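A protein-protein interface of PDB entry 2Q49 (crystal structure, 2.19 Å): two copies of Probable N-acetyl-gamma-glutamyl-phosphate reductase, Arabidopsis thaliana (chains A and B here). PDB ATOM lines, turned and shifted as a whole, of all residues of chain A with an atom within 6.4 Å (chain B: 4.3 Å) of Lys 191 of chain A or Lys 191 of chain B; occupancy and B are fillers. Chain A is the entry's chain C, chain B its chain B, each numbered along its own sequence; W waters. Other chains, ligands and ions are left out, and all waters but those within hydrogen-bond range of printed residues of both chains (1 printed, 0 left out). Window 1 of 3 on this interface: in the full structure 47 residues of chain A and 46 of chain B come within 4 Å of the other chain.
The side-chain carboxylate of Asp 189 of chain B is in salt-bridge range of the side-chain amino group of Lys 191 of chain A (3.0 Å).
The side-chain carboxylate (OD2) of Asp 189 of chain B sits at hydrogen-bond distance from the side-chain hydroxyl (OH) of Tyr 260 of chain A.
The side-chain amino group (NZ) of Lys 191 of chain B lies within salt-bridge range of the side-chain carboxylate (OD1) of Asp 189 of chain A, 3.2 Å away.
NZ of Lys 191 of chain B lies within hydrogen-bond range of NE2 of His 247 of chain A, 3.3 Å away.
OG1 of Thr 297 of chain A lies within hydrogen-bond range of N of Ile 214 of chain B, 2.9 Å away.
NE2 of His 247 of chain B is in hydrogen-bond range of NZ of Lys 191 of chain A.
A ring nitrogen (NE2) of His 247 of chain B sits at hydrogen-bond distance from the side-chain hydroxyl (OG1) of Thr 258 of chain A (3.0 Å).
OG of Ser 216 of chain A is in hydrogen-bond range of NE2 of Gln 256 of chain B (3.0 Å).
The side-chain hydroxyl of Thr 258 of chain B sits at hydrogen-bond distance from a ring nitrogen (NE2) of His 247 of chain A, 3.0 Å away.
OD1 of Asp 189 of chain B sits close to OD1 of Asp 189 of chain A, 3.2 Å away.
The side-chain sulfur (SD) of Met 249 of chain B lies close to the side-chain sulfur (SD) of Met 249 of chain A (3.3 Å).
The backbone carbonyl oxygen (O) of Ala 190 of chain B is in hydrogen-bond range of a ring nitrogen (ND1) of His 247 of chain B (3.0 Å).
The side-chain amide nitrogen (NE2) of Gln 256 of chain B is in hydrogen-bond range of the side-chain hydroxyl (OG1) of Thr 258 of chain B, 3.0 Å away.
NZ of Lys 191 of chain A lies within salt-bridge range of OD1 of Asp 189 of chain A (2.9 Å).
A ring nitrogen (NE2) of His 247 of chain A sits at hydrogen-bond distance from the side-chain hydroxyl (OG) of Ser 216 of chain A (3.1 Å).
The backbone carbonyl oxygen of Thr 245 of chain A sits at hydrogen-bond distance from a ring nitrogen (ND1) of His 247 of chain A (2.9 Å).
NE2 of Gln 256 of chain A sits at hydrogen-bond distance from OG1 of Thr 258 of chain A.
Among the printed residues, pairs that only touch across the chains: Asp 189 of chain A with Thr 258 of chain B, Lys 191 of chain A with Lys 191 of chain B, Lys 191 of chain A with Ile 214 of chain B, Ile 214 of chain A with Lys 191 of chain B, Ile 214 of chain A with Met 249 of chain B, Ser 216 of chain A with Thr 258 of chain B, His 247 of chain A with Gln 256 of chain B, Met 249 of chain A with Ile 214 of chain B, Met 251 of chain A with Ile 214 of chain B, Gln 256 of chain A with Ile 214 of chain B, Gln 256 of chain A with His 247 of chain B and Thr 258 of chain A with Asp 189 of chain B.
Lys 191 of chain A touches just these residues of chain B: Asp 189 (3.0 Å), Lys 191 (3.8 Å), Ile 214 (3.5 Å) and His 247 (3.1 Å).
Printed residues of chain A within 4 Å of Lys 191 of chain B: Asp 189 (3.2 Å), Lys 191 (3.8 Å), Ile 214 (3.5 Å) and His 247 (3.3 Å).
Of the printed residues of chain B, Gln 256 of chain A touches Ile 214 and His 247.
Of the printed residues of chain B, Asp 189 of chain A touches Asp 189 (3.2 Å), Lys 191 (3.2 Å) and Thr 258 (3.5 Å).
Printed residues of chain B within 4 Å of Ile 214 of chain A: Lys 191 (3.5 Å) and Met 249 (3.4 Å).
Of the printed residues of chain B, Thr 258 of chain A touches Asp 189 (3.6 Å) and His 247 (3.0 Å).
Of the printed residues of chain A, Asp 189 of chain B touches Asp 189 (3.2 Å), Lys 191 (3.0 Å), Thr 258 (3.6 Å) and Tyr 260 (2.7 Å).
The nearest printed residue of chain B that does not touch Lys 191 of chain A is Met 249 of chain B (5.2 Å).
Of the 22 printed residues of chain A, 11 touch a printed residue of chain B.
Hydrophobic or aromatic side chains of chain A within 4 Å of the printed part of chain B: Ile 214, His 247, Met 249, Met 251 and Tyr 260.
Among the printed residues, Asp or Glu carboxylates within 4 Å of a Lys or Arg side-chain nitrogen of the other chain: Asp 189 of chain A with Lys 191 of chain B and Lys 191 of chain A with Asp 189 of chain B.
Asp 189 of chain B touches its own counterpart, Asp 189 of chain A.
Asp 189 of chain A touches Lys 191 of chain B, and with the chains exchanged Lys 191 of chain A touches Asp 189 of chain B.
Asp 189 of chain A touches Thr 258 of chain B, and with the chains exchanged Thr 258 of chain A touches Asp 189 of chain B.
Met 249 of chain B touches its own counterpart, Met 249 of chain A.
11 positions are printed for both chains.
Of the 23 pairs that touch across the chains among the printed residues, 17 have their exchanged pair printed and touching as well.
Water W1 bridges OE1 of Gln 256 of chain B (2.7 Å) and N of Ser 216 of chain A (3.2 Å).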
ATOM      1  N   TYR A 164      -4.112  -3.691 -18.396  1.00  0.00           N
ATOM      2  CA  TYR A 164      -2.969  -4.591 -18.498  1.00  0.00           C
ATOM      3  C   TYR A 164      -2.527  -4.785 -19.952  1.00  0.00           C
ATOM      4  O   TYR A 164      -1.350  -4.629 -20.285  1.00  0.00           O
ATOM      5  CB  TYR A 164      -3.311  -5.958 -17.891  1.00  0.00           C
ATOM      6  CG  TYR A 164      -3.424  -5.972 -16.377  1.00  0.00           C
ATOM      7  CD1 TYR A 164      -2.311  -5.722 -15.573  1.00  0.00           C
ATOM      8  CD2 TYR A 164      -4.619  -6.316 -15.753  1.00  0.00           C
ATOM      9  CE1 TYR A 164      -2.380  -5.834 -14.192  1.00  0.00           C
ATOM     10  CE2 TYR A 164      -4.705  -6.429 -14.360  1.00  0.00           C
ATOM     11  CZ  TYR A 164      -3.577  -6.197 -13.590  1.00  0.00           C
ATOM     12  OH  TYR A 164      -3.619  -6.403 -12.228  1.00  0.00           O
ATOM     13  N   ASP A 189       4.196 -10.886 -15.096  1.00  0.00           N
ATOM     14  CA  ASP A 189       3.706 -10.790 -13.727  1.00  0.00           C
ATOM     15  C   ASP A 189       3.267  -9.324 -13.565  1.00  0.00           C
ATOM     16  O   ASP A 189       4.101  -8.422 -13.480  1.00  0.00           O
ATOM     17  CB  ASP A 189       4.808 -11.145 -12.701  1.00  0.00           C
ATOM     18  CG  ASP A 189       4.274 -11.212 -11.275  1.00  0.00           C
ATOM     19  OD1 ASP A 189       3.928 -10.144 -10.715  1.00  0.00           O
ATOM     20  OD2 ASP A 189       4.187 -12.334 -10.718  1.00  0.00           O
ATOM     21  N   ALA A 190       1.953  -9.103 -13.536  1.00  0.00           N
ATOM     22  CA  ALA A 190       1.390  -7.762 -13.445  1.00  0.00           C
ATOM     23  C   ALA A 190       0.832  -7.393 -12.081  1.00  0.00           C
ATOM     24  O   ALA A 190       0.425  -8.250 -11.281  1.00  0.00           O
ATOM     25  CB  ALA A 190       0.323  -7.583 -14.518  1.00  0.00           C
ATOM     26  N   LYS A 191       0.801  -6.090 -11.844  1.00  0.00           N
ATOM     27  CA  LYS A 191       0.356  -5.532 -10.577  1.00  0.00           C
ATOM     28  C   LYS A 191      -0.549  -4.346 -10.844  1.00  0.00           C
ATOM     29  O   LYS A 191      -0.255  -3.519 -11.721  1.00  0.00           O
ATOM     30  CB  LYS A 191       1.574  -5.050  -9.781  1.00  0.00           C
ATOM     31  CG  LYS A 191       2.653  -6.123  -9.437  1.00  0.00           C
ATOM     32  CD  LYS A 191       3.608  -6.468 -10.572  1.00  0.00           C
ATOM     33  CE  LYS A 191       4.760  -7.360 -10.062  1.00  0.00           C
ATOM     34  NZ  LYS A 191       5.682  -7.870 -11.133  1.00  0.00           N
ATOM     35  N   SER A 192      -1.633  -4.238 -10.081  1.00  0.00           N
ATOM     36  CA  SER A 192      -2.556  -3.131 -10.279  1.00  0.00           C
ATOM     37  C   SER A 192      -3.164  -2.587  -9.007  1.00  0.00           C
ATOM     38  O   SER A 192      -3.358  -3.320  -8.044  1.00  0.00           O
ATOM     39  CB  SER A 192      -3.692  -3.548 -11.227  1.00  0.00           C
ATOM     40  OG  SER A 192      -4.670  -2.520 -11.312  1.00  0.00           O
ATOM     41  N   GLY A 193      -3.448  -1.282  -9.013  1.00  0.00           N
ATOM     42  CA  GLY A 193      -4.088  -0.662  -7.877  1.00  0.00           C
ATOM     43  C   GLY A 193      -5.509  -1.206  -7.795  1.00  0.00           C
ATOM     44  O   GLY A 193      -6.059  -1.689  -8.789  1.00  0.00           O
ATOM     45  N   ILE A 214      -0.793  -7.638  -0.565  1.00  0.00           N
ATOM     46  CA  ILE A 214      -1.034  -7.785  -1.991  1.00  0.00           C
ATOM     47  C   ILE A 214      -1.625  -9.166  -2.272  1.00  0.00           C
ATOM     48  O   ILE A 214      -1.582 -10.057  -1.421  1.00  0.00           O
ATOM     49  CB  ILE A 214       0.271  -7.668  -2.837  1.00  0.00           C
ATOM     50  CG1 ILE A 214       1.243  -8.808  -2.490  1.00  0.00           C
ATOM     51  CG2 ILE A 214       0.900  -6.318  -2.647  1.00  0.00           C
ATOM     52  CD1 ILE A 214       2.327  -9.011  -3.564  1.00  0.00           C
ATOM     53  N   SER A 216      -2.576 -12.188  -5.702  1.00  0.00           N
ATOM     54  CA  SER A 216      -2.583 -12.653  -7.069  1.00  0.00           C
ATOM     55  C   SER A 216      -4.062 -12.879  -7.388  1.00  0.00           C
ATOM     56  O   SER A 216      -4.866 -13.059  -6.477  1.00  0.00           O
ATOM     57  CB  SER A 216      -1.854 -13.998  -7.183  1.00  0.00           C
ATOM     58  OG  SER A 216      -0.445 -13.863  -7.104  1.00  0.00           O
ATOM     59  N   TYR A 217      -4.438 -12.845  -8.667  1.00  0.00           N
ATOM     60  CA  TYR A 217      -5.835 -13.125  -9.037  1.00  0.00           C
ATOM     61  C   TYR A 217      -5.853 -13.412 -10.521  1.00  0.00           C
ATOM     62  O   TYR A 217      -4.871 -13.130 -11.206  1.00  0.00           O
ATOM     63  CB  TYR A 217      -6.810 -11.964  -8.682  1.00  0.00           C
ATOM     64  CG  TYR A 217      -6.574 -10.640  -9.403  1.00  0.00           C
ATOM     65  CD1 TYR A 217      -5.588  -9.759  -8.979  1.00  0.00           C
ATOM     66  CD2 TYR A 217      -7.346 -10.275 -10.509  1.00  0.00           C
ATOM     67  CE1 TYR A 217      -5.366  -8.547  -9.629  1.00  0.00           C
ATOM     68  CE2 TYR A 217      -7.138  -9.055 -11.172  1.00  0.00           C
ATOM     69  CZ  TYR A 217      -6.143  -8.203 -10.725  1.00  0.00           C
ATOM     70  OH  TYR A 217      -5.905  -7.027 -11.384  1.00  0.00           O
ATOM     71  N   THR A 245      -0.203 -13.263 -15.123  1.00  0.00           N
ATOM     72  CA  THR A 245      -0.739 -13.342 -13.780  1.00  0.00           C
ATOM     73  C   THR A 245      -0.842 -11.962 -13.157  1.00  0.00           C
ATOM     74  O   THR A 245       0.181 -11.354 -12.810  1.00  0.00           O
ATOM     75  CB  THR A 245       0.168 -14.213 -12.870  1.00  0.00           C
ATOM     76  OG1 THR A 245       0.401 -15.470 -13.499  1.00  0.00           O
ATOM     77  CG2 THR A 245      -0.469 -14.428 -11.509  1.00  0.00           C
ATOM     78  N   PRO A 246      -2.078 -11.447 -13.004  1.00  0.00           N
ATOM     79  CA  PRO A 246      -2.306 -10.120 -12.404  1.00  0.00           C
ATOM     80  C   PRO A 246      -2.095 -10.196 -10.896  1.00  0.00           C
ATOM     81  O   PRO A 246      -2.161 -11.277 -10.317  1.00  0.00           O
ATOM     82  CB  PRO A 246      -3.773  -9.820 -12.731  1.00  0.00           C
ATOM     83  CG  PRO A 246      -4.104 -10.728 -13.863  1.00  0.00           C
ATOM     84  CD  PRO A 246      -3.315 -11.985 -13.594  1.00  0.00           C
ATOM     85  N   HIS A 247      -1.840  -9.049 -10.268  1.00  0.00           N
ATOM     86  CA  HIS A 247      -1.643  -8.972  -8.820  1.00  0.00           C
ATOM     87  C   HIS A 247      -2.260  -7.671  -8.326  1.00  0.00           C
ATOM     88  O   HIS A 247      -1.998  -6.591  -8.879  1.00  0.00           O
ATOM     89  CB  HIS A 247      -0.154  -8.983  -8.442  1.00  0.00           C
ATOM     90  CG  HIS A 247       0.553 -10.271  -8.743  1.00  0.00           C
ATOM     91  ND1 HIS A 247       0.830 -10.687 -10.028  1.00  0.00           N
ATOM     92  CD2 HIS A 247       1.040 -11.233  -7.921  1.00  0.00           C
ATOM     93  CE1 HIS A 247       1.455 -11.854  -9.986  1.00  0.00           C
ATOM     94  NE2 HIS A 247       1.595 -12.206  -8.719  1.00  0.00           N
ATOM     95  N   LEU A 248      -3.045  -7.771  -7.261  1.00  0.00           N
ATOM     96  CA  LEU A 248      -3.736  -6.614  -6.693  1.00  0.00           C
ATOM     97  C   LEU A 248      -2.884  -5.945  -5.627  1.00  0.00           C
ATOM     98  O   LEU A 248      -2.522  -6.585  -4.640  1.00  0.00           O
ATOM     99  CB  LEU A 248      -5.062  -7.064  -6.078  1.00  0.00           C
ATOM    100  CG  LEU A 248      -6.099  -6.005  -5.698  1.00  0.00           C
ATOM    101  CD1 LEU A 248      -6.547  -5.269  -6.953  1.00  0.00           C
ATOM    102  CD2 LEU A 248      -7.292  -6.688  -5.050  1.00  0.00           C
ATOM    103  N   MET A 249      -2.586  -4.658  -5.844  1.00  0.00           N
ATOM    104  CA  MET A 249      -1.778  -3.839  -4.950  1.00  0.00           C
ATOM    105  C   MET A 249      -2.614  -3.015  -3.973  1.00  0.00           C
ATOM    106  O   MET A 249      -3.665  -2.481  -4.345  1.00  0.00           O
ATOM    107  CB  MET A 249      -0.912  -2.863  -5.766  1.00  0.00           C
ATOM    108  CG  MET A 249       0.005  -3.535  -6.788  1.00  0.00           C
ATOM    109  SD  MET A 249       1.298  -4.488  -5.943  1.00  0.00           S
ATOM    110  CE  MET A 249       0.566  -6.176  -6.008  1.00  0.00           C
ATOM    111  N   MET A 251      -3.086  -0.176  -3.192  1.00  0.00           N
ATOM    112  CA  MET A 251      -2.963   1.218  -3.600  1.00  0.00           C
ATOM    113  C   MET A 251      -4.105   1.510  -4.567  1.00  0.00           C
ATOM    114  O   MET A 251      -4.698   0.593  -5.120  1.00  0.00           O
ATOM    115  CB  MET A 251      -1.614   1.470  -4.283  1.00  0.00           C
ATOM    116  CG  MET A 251      -1.433   0.700  -5.594  1.00  0.00           C
ATOM    117  SD  MET A 251       0.279   0.694  -6.136  1.00  0.00           S
ATOM    118  CE  MET A 251       0.139   0.129  -7.823  1.00  0.00           C
ATOM    119  N   GLY A 254      -2.222   2.971 -10.500  1.00  0.00           N
ATOM    120  CA  GLY A 254      -0.931   2.414 -10.838  1.00  0.00           C
ATOM    121  C   GLY A 254      -0.979   0.989 -11.333  1.00  0.00           C
ATOM    122  O   GLY A 254      -1.782   0.168 -10.884  1.00  0.00           O
ATOM    123  N   MET A 255      -0.096   0.694 -12.266  1.00  0.00           N
ATOM    124  CA  MET A 255      -0.055  -0.628 -12.823  1.00  0.00           C
ATOM    125  C   MET A 255       1.291  -0.952 -13.427  1.00  0.00           C
ATOM    126  O   MET A 255       1.881  -0.151 -14.165  1.00  0.00           O
ATOM    127  CB  MET A 255      -1.138  -0.777 -13.895  1.00  0.00           C
ATOM    128  CG  MET A 255      -1.103  -2.103 -14.632  1.00  0.00           C
ATOM    129  SD  MET A 255      -2.442  -2.232 -15.820  1.00  0.00           S
ATOM    130  CE  MET A 255      -3.786  -2.646 -14.739  1.00  0.00           C
ATOM    131  N   GLN A 256       1.781  -2.141 -13.098  1.00  0.00           N
ATOM    132  CA  GLN A 256       3.030  -2.596 -13.652  1.00  0.00           C
ATOM    133  C   GLN A 256       2.914  -4.026 -14.104  1.00  0.00           C
ATOM    134  O   GLN A 256       2.403  -4.880 -13.377  1.00  0.00           O
ATOM    135  CB  GLN A 256       4.183  -2.523 -12.651  1.00  0.00           C
ATOM    136  CG  GLN A 256       5.525  -2.964 -13.297  1.00  0.00           C
ATOM    137  CD  GLN A 256       6.712  -2.902 -12.349  1.00  0.00           C
ATOM    138  OE1 GLN A 256       6.970  -1.882 -11.708  1.00  0.00           O
ATOM    139  NE2 GLN A 256       7.446  -3.997 -12.270  1.00  0.00           N
ATOM    140  N   SER A 257       3.383  -4.274 -15.314  1.00  0.00           N
ATOM    141  CA  SER A 257       3.412  -5.621 -15.842  1.00  0.00           C
ATOM    142  C   SER A 257       4.876  -5.997 -16.098  1.00  0.00           C
ATOM    143  O   SER A 257       5.404  -5.697 -17.167  1.00  0.00           O
ATOM    144  CB  SER A 257       2.600  -5.715 -17.139  1.00  0.00           C
ATOM    145  OG  SER A 257       1.211  -5.634 -16.849  1.00  0.00           O
ATOM    146  N   THR A 258       5.534  -6.606 -15.100  1.00  0.00           N
ATOM    147  CA  THR A 258       6.926  -7.049 -15.254  1.00  0.00           C
ATOM    148  C   THR A 258       6.880  -8.196 -16.271  1.00  0.00           C
ATOM    149  O   THR A 258       6.268  -9.234 -16.023  1.00  0.00           O
ATOM    150  CB  THR A 258       7.549  -7.571 -13.933  1.00  0.00           C
ATOM    151  OG1 THR A 258       7.442  -6.569 -12.903  1.00  0.00           O
ATOM    152  CG2 THR A 258       9.046  -7.904 -14.161  1.00  0.00           C
ATOM    153  N   TYR A 260       8.802 -10.989 -18.725  1.00  0.00           N
ATOM    154  CA  TYR A 260       9.990 -11.815 -18.923  1.00  0.00           C
ATOM    155  C   TYR A 260       9.877 -12.484 -20.294  1.00  0.00           C
ATOM    156  O   TYR A 260       8.955 -13.269 -20.546  1.00  0.00           O
ATOM    157  CB  TYR A 260      10.079 -12.872 -17.819  1.00  0.00           C
ATOM    158  CG  TYR A 260      10.053 -12.299 -16.418  1.00  0.00           C
ATOM    159  CD1 TYR A 260      11.238 -11.926 -15.771  1.00  0.00           C
ATOM    160  CD2 TYR A 260       8.833 -12.100 -15.745  1.00  0.00           C
ATOM    161  CE1 TYR A 260      11.215 -11.366 -14.493  1.00  0.00           C
ATOM    162  CE2 TYR A 260       8.795 -11.540 -14.465  1.00  0.00           C
ATOM    163  CZ  TYR A 260       9.987 -11.169 -13.843  1.00  0.00           C
ATOM    164  OH  TYR A 260       9.973 -10.566 -12.594  1.00  0.00           O
ATOM    165  N   THR A 297       5.554   3.183 -10.646  1.00  0.00           N
ATOM    166  CA  THR A 297       4.189   3.631 -10.945  1.00  0.00           C
ATOM    167  C   THR A 297       3.987   5.036 -10.341  1.00  0.00           C
ATOM    168  O   THR A 297       3.023   5.719 -10.653  1.00  0.00           O
ATOM    169  CB  THR A 297       3.104   2.686 -10.356  1.00  0.00           C
ATOM    170  OG1 THR A 297       3.179   2.703  -8.926  1.00  0.00           O
ATOM    171  CG2 THR A 297       3.283   1.267 -10.878  1.00  0.00           C
ATOM    172  N   TYR B 164      13.362 -13.351   1.149  1.00  0.00           N
ATOM    173  CA  TYR B 164      12.962 -13.821  -0.165  1.00  0.00           C
ATOM    174  C   TYR B 164      13.375 -15.296  -0.369  1.00  0.00           C
ATOM    175  O   TYR B 164      12.532 -16.124  -0.725  1.00  0.00           O
ATOM    176  CB  TYR B 164      13.556 -12.932  -1.268  1.00  0.00           C
ATOM    177  CG  TYR B 164      12.906 -11.557  -1.418  1.00  0.00           C
ATOM    178  CD1 TYR B 164      11.607 -11.431  -1.907  1.00  0.00           C
ATOM    179  CD2 TYR B 164      13.617 -10.389  -1.137  1.00  0.00           C
ATOM    180  CE1 TYR B 164      11.020 -10.172  -2.129  1.00  0.00           C
ATOM    181  CE2 TYR B 164      13.053  -9.113  -1.346  1.00  0.00           C
ATOM    182  CZ  TYR B 164      11.747  -9.014  -1.848  1.00  0.00           C
ATOM    183  OH  TYR B 164      11.169  -7.771  -2.085  1.00  0.00           O
ATOM    184  N   ASP B 189       9.242 -13.848  -9.268  1.00  0.00           N
ATOM    185  CA  ASP B 189       8.786 -12.468  -9.191  1.00  0.00           C
ATOM    186  C   ASP B 189       8.243 -12.308  -7.768  1.00  0.00           C
ATOM    187  O   ASP B 189       7.130 -12.743  -7.477  1.00  0.00           O
ATOM    188  CB  ASP B 189       7.681 -12.216 -10.229  1.00  0.00           C
ATOM    189  CG  ASP B 189       7.342 -10.738 -10.360  1.00  0.00           C
ATOM    190  OD1 ASP B 189       6.876 -10.172  -9.354  1.00  0.00           O
ATOM    191  OD2 ASP B 189       7.562 -10.157 -11.449  1.00  0.00           O
ATOM    192  N   ALA B 190       9.041 -11.712  -6.876  1.00  0.00           N
ATOM    193  CA  ALA B 190       8.636 -11.554  -5.487  1.00  0.00           C
ATOM    194  C   ALA B 190       8.310 -10.134  -5.048  1.00  0.00           C
ATOM    195  O   ALA B 190       8.648  -9.151  -5.724  1.00  0.00           O
ATOM    196  CB  ALA B 190       9.706 -12.162  -4.557  1.00  0.00           C
ATOM    197  N   LYS B 191       7.648 -10.038  -3.899  1.00  0.00           N
ATOM    198  CA  LYS B 191       7.226  -8.750  -3.340  1.00  0.00           C
ATOM    199  C   LYS B 191       7.321  -8.736  -1.822  1.00  0.00           C
ATOM    200  O   LYS B 191       6.966  -9.705  -1.138  1.00  0.00           O
ATOM    201  CB  LYS B 191       5.769  -8.452  -3.716  1.00  0.00           C
ATOM    202  CG  LYS B 191       5.468  -8.469  -5.207  1.00  0.00           C
ATOM    203  CD  LYS B 191       5.203  -9.875  -5.728  1.00  0.00           C
ATOM    204  CE  LYS B 191       4.766  -9.823  -7.177  1.00  0.00           C
ATOM    205  NZ  LYS B 191       4.617 -11.172  -7.807  1.00  0.00           N
ATOM    206  N   SER B 192       7.769  -7.613  -1.288  1.00  0.00           N
ATOM    207  CA  SER B 192       7.860  -7.476   0.146  1.00  0.00           C
ATOM    208  C   SER B 192       7.454  -6.070   0.568  1.00  0.00           C
ATOM    209  O   SER B 192       7.589  -5.110  -0.196  1.00  0.00           O
ATOM    210  CB  SER B 192       9.284  -7.761   0.639  1.00  0.00           C
ATOM    211  OG  SER B 192       9.270  -8.150   2.014  1.00  0.00           O
ATOM    212  N   ILE B 214       4.350   1.204  -6.772  1.00  0.00           N
ATOM    213  CA  ILE B 214       5.301   0.108  -6.709  1.00  0.00           C
ATOM    214  C   ILE B 214       6.395   0.299  -7.761  1.00  0.00           C
ATOM    215  O   ILE B 214       6.311   1.189  -8.618  1.00  0.00           O
ATOM    216  CB  ILE B 214       4.655  -1.283  -6.974  1.00  0.00           C
ATOM    217  CG1 ILE B 214       4.236  -1.398  -8.443  1.00  0.00           C
ATOM    218  CG2 ILE B 214       3.486  -1.516  -6.037  1.00  0.00           C
ATOM    219  CD1 ILE B 214       4.109  -2.847  -8.875  1.00  0.00           C
ATOM    220  N   HIS B 247      10.390  -6.470  -5.705  1.00  0.00           N
ATOM    221  CA  HIS B 247       9.469  -5.348  -5.939  1.00  0.00           C
ATOM    222  C   HIS B 247       9.148  -4.755  -4.564  1.00  0.00           C
ATOM    223  O   HIS B 247       9.008  -5.489  -3.578  1.00  0.00           O
ATOM    224  CB  HIS B 247       8.166  -5.815  -6.613  1.00  0.00           C
ATOM    225  CG  HIS B 247       8.354  -6.390  -7.984  1.00  0.00           C
ATOM    226  ND1 HIS B 247       8.992  -7.593  -8.208  1.00  0.00           N
ATOM    227  CD2 HIS B 247       8.002  -5.923  -9.206  1.00  0.00           C
ATOM    228  CE1 HIS B 247       9.024  -7.844  -9.504  1.00  0.00           C
ATOM    229  NE2 HIS B 247       8.430  -6.845 -10.135  1.00  0.00           N
ATOM    230  N   MET B 249       6.585  -2.991  -2.154  1.00  0.00           N
ATOM    231  CA  MET B 249       5.148  -2.802  -1.940  1.00  0.00           C
ATOM    232  C   MET B 249       4.785  -1.687  -0.961  1.00  0.00           C
ATOM    233  O   MET B 249       5.445  -1.511   0.061  1.00  0.00           O
ATOM    234  CB  MET B 249       4.522  -4.101  -1.424  1.00  0.00           C
ATOM    235  CG  MET B 249       4.706  -5.302  -2.340  1.00  0.00           C
ATOM    236  SD  MET B 249       3.837  -5.206  -3.941  1.00  0.00           S
ATOM    237  CE  MET B 249       5.202  -4.855  -5.093  1.00  0.00           C
ATOM    238  N   MET B 255       5.094 -10.474   2.731  1.00  0.00           N
ATOM    239  CA  MET B 255       5.968 -10.896   1.642  1.00  0.00           C
ATOM    240  C   MET B 255       5.428 -12.101   0.883  1.00  0.00           C
ATOM    241  O   MET B 255       5.082 -13.142   1.470  1.00  0.00           O
ATOM    242  CB  MET B 255       7.375 -11.229   2.188  1.00  0.00           C
ATOM    243  CG  MET B 255       8.265 -12.009   1.244  1.00  0.00           C
ATOM    244  SD  MET B 255       9.953 -12.134   1.885  1.00  0.00           S
ATOM    245  CE  MET B 255      10.670 -10.616   1.361  1.00  0.00           C
ATOM    246  N   GLN B 256       5.370 -11.962  -0.430  1.00  0.00           N
ATOM    247  CA  GLN B 256       4.896 -13.042  -1.267  1.00  0.00           C
ATOM    248  C   GLN B 256       5.930 -13.320  -2.329  1.00  0.00           C
ATOM    249  O   GLN B 256       6.745 -12.456  -2.620  1.00  0.00           O
ATOM    250  CB  GLN B 256       3.573 -12.669  -1.956  1.00  0.00           C
ATOM    251  CG  GLN B 256       3.246 -13.571  -3.157  1.00  0.00           C
ATOM    252  CD  GLN B 256       1.811 -13.414  -3.691  1.00  0.00           C
ATOM    253  OE1 GLN B 256       0.840 -13.296  -2.927  1.00  0.00           O
ATOM    254  NE2 GLN B 256       1.680 -13.455  -5.006  1.00  0.00           N
ATOM    255  N   THR B 258       5.954 -15.053  -6.280  1.00  0.00           N
ATOM    256  CA  THR B 258       5.236 -15.722  -7.355  1.00  0.00           C
ATOM    257  C   THR B 258       6.299 -16.435  -8.192  1.00  0.00           C
ATOM    258  O   THR B 258       7.134 -15.805  -8.855  1.00  0.00           O
ATOM    259  CB  THR B 258       4.394 -14.738  -8.208  1.00  0.00           C
ATOM    260  OG1 THR B 258       3.506 -14.009  -7.348  1.00  0.00           O
ATOM    261  CG2 THR B 258       3.546 -15.514  -9.229  1.00  0.00           C
HETATM  262  O   HOH W   1      -1.387 -14.528  -3.823  1.00  0.00           O
